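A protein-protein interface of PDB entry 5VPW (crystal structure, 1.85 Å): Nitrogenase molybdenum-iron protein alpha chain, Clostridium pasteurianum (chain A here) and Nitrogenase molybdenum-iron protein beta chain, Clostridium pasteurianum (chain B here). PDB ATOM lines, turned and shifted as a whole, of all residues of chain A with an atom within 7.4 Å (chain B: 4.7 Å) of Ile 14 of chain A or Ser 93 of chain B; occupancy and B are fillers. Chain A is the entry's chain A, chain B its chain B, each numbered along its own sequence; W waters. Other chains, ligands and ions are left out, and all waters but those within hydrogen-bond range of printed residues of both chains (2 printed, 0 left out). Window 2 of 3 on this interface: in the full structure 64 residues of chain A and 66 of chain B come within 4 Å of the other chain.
O of Ser 93 of chain B touches CE of Lys 12 of chain A, 3.5 Å away.
Leu 94 of chain B touches Tyr 13 of chain A (CD1 to CE1, 3.8 Å).
Ile 14 of chain A touches Asn 90 of chain B (CG1 to OD1, 3.8 Å).
Ile 14 of chain A touches Ser 93 of chain B (CG2 to OG, 3.3 Å).
Asn 90 of chain B touches Val 44 of chain A.
CD2 of Leu 94 of chain B touches ND1 of His 447 of chain A, 3.7 Å away.
NZ of Lys 12 of chain A sits at hydrogen-bond distance from O of Leu 94 of chain B.
OG1 of Thr 17 of chain A lies within hydrogen-bond range of OD1 of Asn 90 of chain B, 2.7 Å away.
The side-chain hydroxyl of Tyr 95 of chain B is in hydrogen-bond range of the backbone NH of His 447 of chain A, 3.0 Å away.
Of chain B, only Asn 90 (3.8 Å) and Ser 93 (3.3 Å) come within 4 Å of Ile 14 of chain A.
Ser 93 of chain B touches just these residues of chain A: Lys 12 and Ile 14.
Printed residues of chain B within 4 Å of Tyr 13 of chain A: Leu 94 (3.8 Å).
Of the printed residues of chain B, His 447 of chain A touches Leu 94 and Tyr 95.
The nearest residue of chain B that does not touch Ile 14 of chain A is Lys 89 of chain B (4.2 Å).
Water W1 lies within hydrogen-bond range of OG1 of Thr 17 of chain A (2.6 Å) and ND2 of Asn 90 of chain B (3.1 Å).
Water W2 lies within hydrogen-bond range of N of Ile 14 of chain A (2.9 Å), OD1 of Asn 90 of chain B (2.9 Å) and OG of Ser 93 of chain B (3.4 Å).
Hydrophobic or aromatic side chains of chain A within 4 Å of the printed part of chain B: Tyr 13, Ile 14, Val 44 and His 447.
Along chain A the printed residues that touch a printed residue of chain B span positions 12 to 447.
Hydrophobic or aromatic side chains of chain B within 4 Å of the printed part of chain A: Leu 94 and Tyr 95.
Along chain B the printed residues that touch a printed residue of chain A span positions 90 to 95.
Among the printed residues, 9 pairs touch across the chains.
Among the printed residues, no Asp or Glu carboxylate lies within 4 Å of a Lys or Arg side-chain nitrogen of the other chain.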
ATOM      1  N   LEU A  10      -1.173 -25.929   2.724  1.00  0.00           N
ATOM      2  CA  LEU A  10      -2.417 -25.857   3.500  1.00  0.00           C
ATOM      3  C   LEU A  10      -2.202 -25.737   5.012  1.00  0.00           C
ATOM      4  O   LEU A  10      -3.106 -25.308   5.748  1.00  0.00           O
ATOM      5  CB  LEU A  10      -3.274 -27.093   3.213  1.00  0.00           C
ATOM      6  CG  LEU A  10      -3.959 -27.182   1.859  1.00  0.00           C
ATOM      7  CD1 LEU A  10      -4.589 -28.573   1.666  1.00  0.00           C
ATOM      8  CD2 LEU A  10      -4.996 -26.072   1.726  1.00  0.00           C
ATOM      9  N   GLU A  11      -1.018 -26.142   5.481  1.00  0.00           N
ATOM     10  CA  GLU A  11      -0.809 -26.368   6.934  1.00  0.00           C
ATOM     11  C   GLU A  11      -1.134 -25.167   7.827  1.00  0.00           C
ATOM     12  O   GLU A  11      -1.751 -25.320   8.863  1.00  0.00           O
ATOM     13  CB  GLU A  11       0.623 -26.830   7.199  1.00  0.00           C
ATOM     14  CG  GLU A  11       0.886 -27.247   8.648  1.00  0.00           C
ATOM     15  CD  GLU A  11       2.187 -28.051   8.801  1.00  0.00           C
ATOM     16  OE1 GLU A  11       3.138 -27.503   9.379  1.00  0.00           O
ATOM     17  OE2 GLU A  11       2.278 -29.217   8.337  1.00  0.00           O
ATOM     18  N   LYS A  12      -0.733 -23.973   7.428  1.00  0.00           N
ATOM     19  CA  LYS A  12      -0.887 -22.787   8.293  1.00  0.00           C
ATOM     20  C   LYS A  12      -2.286 -22.208   8.325  1.00  0.00           C
ATOM     21  O   LYS A  12      -2.571 -21.371   9.150  1.00  0.00           O
ATOM     22  CB  LYS A  12       0.072 -21.691   7.833  1.00  0.00           C
ATOM     23  CG  LYS A  12       0.276 -20.559   8.838  1.00  0.00           C
ATOM     24  CD  LYS A  12       1.350 -19.623   8.324  1.00  0.00           C
ATOM     25  CE  LYS A  12       1.720 -18.582   9.367  1.00  0.00           C
ATOM     26  NZ  LYS A  12       2.575 -17.518   8.758  1.00  0.00           N
ATOM     27  N   TYR A  13      -3.156 -22.607   7.402  1.00  0.00           N
ATOM     28  CA  TYR A  13      -4.510 -22.069   7.370  1.00  0.00           C
ATOM     29  C   TYR A  13      -5.298 -22.491   8.620  1.00  0.00           C
ATOM     30  O   TYR A  13      -5.192 -23.635   9.051  1.00  0.00           O
ATOM     31  CB  TYR A  13      -5.279 -22.612   6.177  1.00  0.00           C
ATOM     32  CG  TYR A  13      -4.943 -22.079   4.779  1.00  0.00           C
ATOM     33  CD1 TYR A  13      -4.888 -20.724   4.506  1.00  0.00           C
ATOM     34  CD2 TYR A  13      -4.724 -22.956   3.730  1.00  0.00           C
ATOM     35  CE1 TYR A  13      -4.610 -20.257   3.217  1.00  0.00           C
ATOM     36  CE2 TYR A  13      -4.444 -22.504   2.445  1.00  0.00           C
ATOM     37  CZ  TYR A  13      -4.381 -21.152   2.190  1.00  0.00           C
ATOM     38  OH  TYR A  13      -4.161 -20.705   0.883  1.00  0.00           O
ATOM     39  N   ILE A  14      -6.137 -21.600   9.149  1.00  0.00           N
ATOM     40  CA  ILE A  14      -7.051 -22.000  10.206  1.00  0.00           C
ATOM     41  C   ILE A  14      -8.018 -23.079   9.673  1.00  0.00           C
ATOM     42  O   ILE A  14      -8.230 -23.218   8.470  1.00  0.00           O
ATOM     43  CB  ILE A  14      -7.773 -20.790  10.843  1.00  0.00           C
ATOM     44  CG1 ILE A  14      -8.676 -20.062   9.817  1.00  0.00           C
ATOM     45  CG2 ILE A  14      -6.728 -19.863  11.455  1.00  0.00           C
ATOM     46  CD1 ILE A  14      -9.558 -18.964  10.408  1.00  0.00           C
ATOM     47  N   PRO A  15      -8.586 -23.892  10.570  1.00  0.00           N
ATOM     48  CA  PRO A  15      -9.416 -25.027  10.120  1.00  0.00           C
ATOM     49  C   PRO A  15     -10.502 -24.737   9.051  1.00  0.00           C
ATOM     50  O   PRO A  15     -10.590 -25.459   8.057  1.00  0.00           O
ATOM     51  CB  PRO A  15     -10.065 -25.508  11.447  1.00  0.00           C
ATOM     52  CG  PRO A  15      -8.996 -25.210  12.471  1.00  0.00           C
ATOM     53  CD  PRO A  15      -8.365 -23.904  12.036  1.00  0.00           C
ATOM     54  N   LYS A  16     -11.338 -23.729   9.276  1.00  0.00           N
ATOM     55  CA  LYS A  16     -12.388 -23.352   8.329  1.00  0.00           C
ATOM     56  C   LYS A  16     -11.815 -22.996   6.933  1.00  0.00           C
ATOM     57  O   LYS A  16     -12.342 -23.385   5.901  1.00  0.00           O
ATOM     58  CB  LYS A  16     -13.148 -22.147   8.865  1.00  0.00           C
ATOM     59  CG  LYS A  16     -14.284 -21.688   7.967  1.00  0.00           C
ATOM     60  CD  LYS A  16     -15.143 -20.625   8.659  1.00  0.00           C
ATOM     61  CE  LYS A  16     -15.921 -19.821   7.619  1.00  0.00           C
ATOM     62  NZ  LYS A  16     -16.809 -18.796   8.243  1.00  0.00           N
ATOM     63  N   THR A  17     -10.745 -22.233   6.931  1.00  0.00           N
ATOM     64  CA  THR A  17     -10.098 -21.856   5.710  1.00  0.00           C
ATOM     65  C   THR A  17      -9.396 -23.025   5.031  1.00  0.00           C
ATOM     66  O   THR A  17      -9.468 -23.171   3.821  1.00  0.00           O
ATOM     67  CB  THR A  17      -9.107 -20.714   5.966  1.00  0.00           C
ATOM     68  OG1 THR A  17      -9.838 -19.598   6.479  1.00  0.00           O
ATOM     69  CG2 THR A  17      -8.406 -20.300   4.647  1.00  0.00           C
ATOM     70  N   LYS A  18      -8.716 -23.856   5.799  1.00  0.00           N
ATOM     71  CA  LYS A  18      -8.017 -25.013   5.235  1.00  0.00           C
ATOM     72  C   LYS A  18      -9.009 -25.898   4.504  1.00  0.00           C
ATOM     73  O   LYS A  18      -8.745 -26.346   3.391  1.00  0.00           O
ATOM     74  CB  LYS A  18      -7.326 -25.802   6.357  1.00  0.00           C
ATOM     75  CG  LYS A  18      -6.368 -26.881   5.885  1.00  0.00           C
ATOM     76  CD  LYS A  18      -5.772 -27.643   7.071  1.00  0.00           C
ATOM     77  CE  LYS A  18      -4.705 -28.611   6.579  1.00  0.00           C
ATOM     78  NZ  LYS A  18      -4.125 -29.433   7.681  1.00  0.00           N
ATOM     79  N   LYS A  19     -10.166 -26.133   5.121  1.00  0.00           N
ATOM     80  CA  LYS A  19     -11.183 -26.986   4.511  1.00  0.00           C
ATOM     81  C   LYS A  19     -11.675 -26.421   3.171  1.00  0.00           C
ATOM     82  O   LYS A  19     -11.815 -27.149   2.215  1.00  0.00           O
ATOM     83  CB  LYS A  19     -12.364 -27.194   5.476  1.00  0.00           C
ATOM     84  CG  LYS A  19     -13.576 -27.893   4.858  1.00  0.00           C
ATOM     85  CD  LYS A  19     -14.371 -28.689   5.891  1.00  0.00           C
ATOM     86  CE  LYS A  19     -15.119 -29.865   5.263  1.00  0.00           C
ATOM     87  NZ  LYS A  19     -15.277 -31.001   6.219  1.00  0.00           N
ATOM     88  N   THR A  20     -11.918 -25.122   3.101  1.00  0.00           N
ATOM     89  CA  THR A  20     -12.380 -24.524   1.854  1.00  0.00           C
ATOM     90  C   THR A  20     -11.258 -24.475   0.768  1.00  0.00           C
ATOM     91  O   THR A  20     -11.529 -24.686  -0.405  1.00  0.00           O
ATOM     92  CB  THR A  20     -13.029 -23.146   2.128  1.00  0.00           C
ATOM     93  OG1 THR A  20     -13.743 -22.710   0.978  1.00  0.00           O
ATOM     94  CG2 THR A  20     -12.034 -22.118   2.450  1.00  0.00           C
ATOM     95  N   VAL A  44     -11.716 -15.964  -0.121  1.00  0.00           N
ATOM     96  CA  VAL A  44     -11.718 -15.893   1.367  1.00  0.00           C
ATOM     97  C   VAL A  44     -11.270 -14.496   1.785  1.00  0.00           C
ATOM     98  O   VAL A  44     -10.193 -14.046   1.386  1.00  0.00           O
ATOM     99  CB  VAL A  44     -10.779 -16.947   1.993  1.00  0.00           C
ATOM    100  CG1 VAL A  44     -10.666 -16.739   3.491  1.00  0.00           C
ATOM    101  CG2 VAL A  44     -11.235 -18.370   1.647  1.00  0.00           C
ATOM    102  N   HIS A 447       0.257 -16.139   0.719  1.00  0.00           N
ATOM    103  CA  HIS A 447       0.714 -17.253   1.538  1.00  0.00           C
ATOM    104  C   HIS A 447       1.111 -18.434   0.649  1.00  0.00           C
ATOM    105  O   HIS A 447       2.220 -18.950   0.797  1.00  0.00           O
ATOM    106  CB  HIS A 447      -0.377 -17.709   2.543  1.00  0.00           C
ATOM    107  CG  HIS A 447      -0.124 -19.074   3.102  1.00  0.00           C
ATOM    108  ND1 HIS A 447       0.767 -19.295   4.127  1.00  0.00           N
ATOM    109  CD2 HIS A 447      -0.577 -20.293   2.729  1.00  0.00           C
ATOM    110  CE1 HIS A 447       0.835 -20.586   4.383  1.00  0.00           C
ATOM    111  NE2 HIS A 447       0.024 -21.215   3.551  1.00  0.00           N
ATOM    112  N   LYS B  89      -9.692 -12.800  11.270  1.00  0.00           N
ATOM    113  CA  LYS B  89      -9.268 -14.147  11.693  1.00  0.00           C
ATOM    114  C   LYS B  89      -8.173 -14.712  10.793  1.00  0.00           C
ATOM    115  O   LYS B  89      -7.202 -15.313  11.259  1.00  0.00           O
ATOM    116  CB  LYS B  89     -10.461 -15.113  11.705  1.00  0.00           C
ATOM    117  CG  LYS B  89     -11.429 -14.844  12.832  1.00  0.00           C
ATOM    118  CD  LYS B  89     -12.724 -15.636  12.717  1.00  0.00           C
ATOM    119  CE  LYS B  89     -13.240 -15.954  14.111  1.00  0.00           C
ATOM    120  NZ  LYS B  89     -14.718 -15.872  14.201  1.00  0.00           N
ATOM    121  N   ASN B  90      -8.339 -14.555   9.487  1.00  0.00           N
ATOM    122  CA  ASN B  90      -7.337 -15.070   8.563  1.00  0.00           C
ATOM    123  C   ASN B  90      -6.074 -14.222   8.550  1.00  0.00           C
ATOM    124  O   ASN B  90      -4.977 -14.747   8.334  1.00  0.00           O
ATOM    125  CB  ASN B  90      -7.904 -15.158   7.162  1.00  0.00           C
ATOM    126  CG  ASN B  90      -8.808 -16.343   7.002  1.00  0.00           C
ATOM    127  OD1 ASN B  90      -8.346 -17.472   7.009  1.00  0.00           O
ATOM    128  ND2 ASN B  90     -10.097 -16.094   6.854  1.00  0.00           N
ATOM    129  N   ILE B  91      -6.222 -12.924   8.773  1.00  0.00           N
ATOM    130  CA  ILE B  91      -5.074 -12.026   8.689  1.00  0.00           C
ATOM    131  C   ILE B  91      -4.112 -12.292   9.830  1.00  0.00           C
ATOM    132  O   ILE B  91      -2.929 -12.519   9.590  1.00  0.00           O
ATOM    133  CB  ILE B  91      -5.473 -10.547   8.636  1.00  0.00           C
ATOM    134  CG1 ILE B  91      -6.141 -10.202   7.280  1.00  0.00           C
ATOM    135  CG2 ILE B  91      -4.269  -9.637   8.866  1.00  0.00           C
ATOM    136  CD1 ILE B  91      -6.992  -8.956   7.328  1.00  0.00           C
ATOM    137  N   PHE B  92      -4.594 -12.291  11.068  1.00  0.00           N
ATOM    138  CA  PHE B  92      -3.675 -12.468  12.191  1.00  0.00           C
ATOM    139  C   PHE B  92      -2.966 -13.815  12.142  1.00  0.00           C
ATOM    140  O   PHE B  92      -1.782 -13.866  12.383  1.00  0.00           O
ATOM    141  CB  PHE B  92      -4.343 -12.187  13.560  1.00  0.00           C
ATOM    142  CG  PHE B  92      -4.523 -10.729  13.849  1.00  0.00           C
ATOM    143  CD1 PHE B  92      -3.431  -9.868  13.854  1.00  0.00           C
ATOM    144  CD2 PHE B  92      -5.780 -10.203  14.073  1.00  0.00           C
ATOM    145  CE1 PHE B  92      -3.602  -8.529  14.079  1.00  0.00           C
ATOM    146  CE2 PHE B  92      -5.954  -8.863  14.313  1.00  0.00           C
ATOM    147  CZ  PHE B  92      -4.869  -8.021  14.314  1.00  0.00           C
ATOM    148  N   SER B  93      -3.646 -14.880  11.732  1.00  0.00           N
ATOM    149  CA  SER B  93      -3.046 -16.227  11.708  1.00  0.00           C
ATOM    150  C   SER B  93      -2.168 -16.451  10.504  1.00  0.00           C
ATOM    151  O   SER B  93      -1.111 -17.049  10.643  1.00  0.00           O
ATOM    152  CB  SER B  93      -4.086 -17.360  11.718  1.00  0.00           C
ATOM    153  OG  SER B  93      -4.537 -17.652  10.390  1.00  0.00           O
ATOM    154  N   LEU B  94      -2.571 -15.985   9.327  1.00  0.00           N
ATOM    155  CA  LEU B  94      -1.729 -16.213   8.152  1.00  0.00           C
ATOM    156  C   LEU B  94      -0.543 -15.269   8.069  1.00  0.00           C
ATOM    157  O   LEU B  94       0.535 -15.686   7.692  1.00  0.00           O
ATOM    158  CB  LEU B  94      -2.510 -16.097   6.858  1.00  0.00           C
ATOM    159  CG  LEU B  94      -3.143 -17.363   6.316  1.00  0.00           C
ATOM    160  CD1 LEU B  94      -3.724 -16.990   4.973  1.00  0.00           C
ATOM    161  CD2 LEU B  94      -2.180 -18.522   6.188  1.00  0.00           C
ATOM    162  N   TYR B  95      -0.756 -14.005   8.416  1.00  0.00           N
ATOM    163  CA  TYR B  95       0.207 -12.956   8.067  1.00  0.00           C
ATOM    164  C   TYR B  95       0.728 -12.165   9.258  1.00  0.00           C
ATOM    165  O   TYR B  95       1.682 -11.416   9.116  1.00  0.00           O
ATOM    166  CB  TYR B  95      -0.426 -12.011   7.011  1.00  0.00           C
ATOM    167  CG  TYR B  95      -0.843 -12.741   5.737  1.00  0.00           C
ATOM    168  CD1 TYR B  95       0.106 -13.427   4.963  1.00  0.00           C
ATOM    169  CD2 TYR B  95      -2.168 -12.791   5.326  1.00  0.00           C
ATOM    170  CE1 TYR B  95      -0.255 -14.100   3.820  1.00  0.00           C
ATOM    171  CE2 TYR B  95      -2.532 -13.470   4.169  1.00  0.00           C
ATOM    172  CZ  TYR B  95      -1.577 -14.137   3.417  1.00  0.00           C
ATOM    173  OH  TYR B  95      -1.932 -14.814   2.247  1.00  0.00           O
HETATM  174  O   HOH W   1     -12.159 -18.470   6.888  1.00  0.00           O
HETATM  175  O   HOH W   2      -5.994 -19.092   7.711  1.00  0.00           O
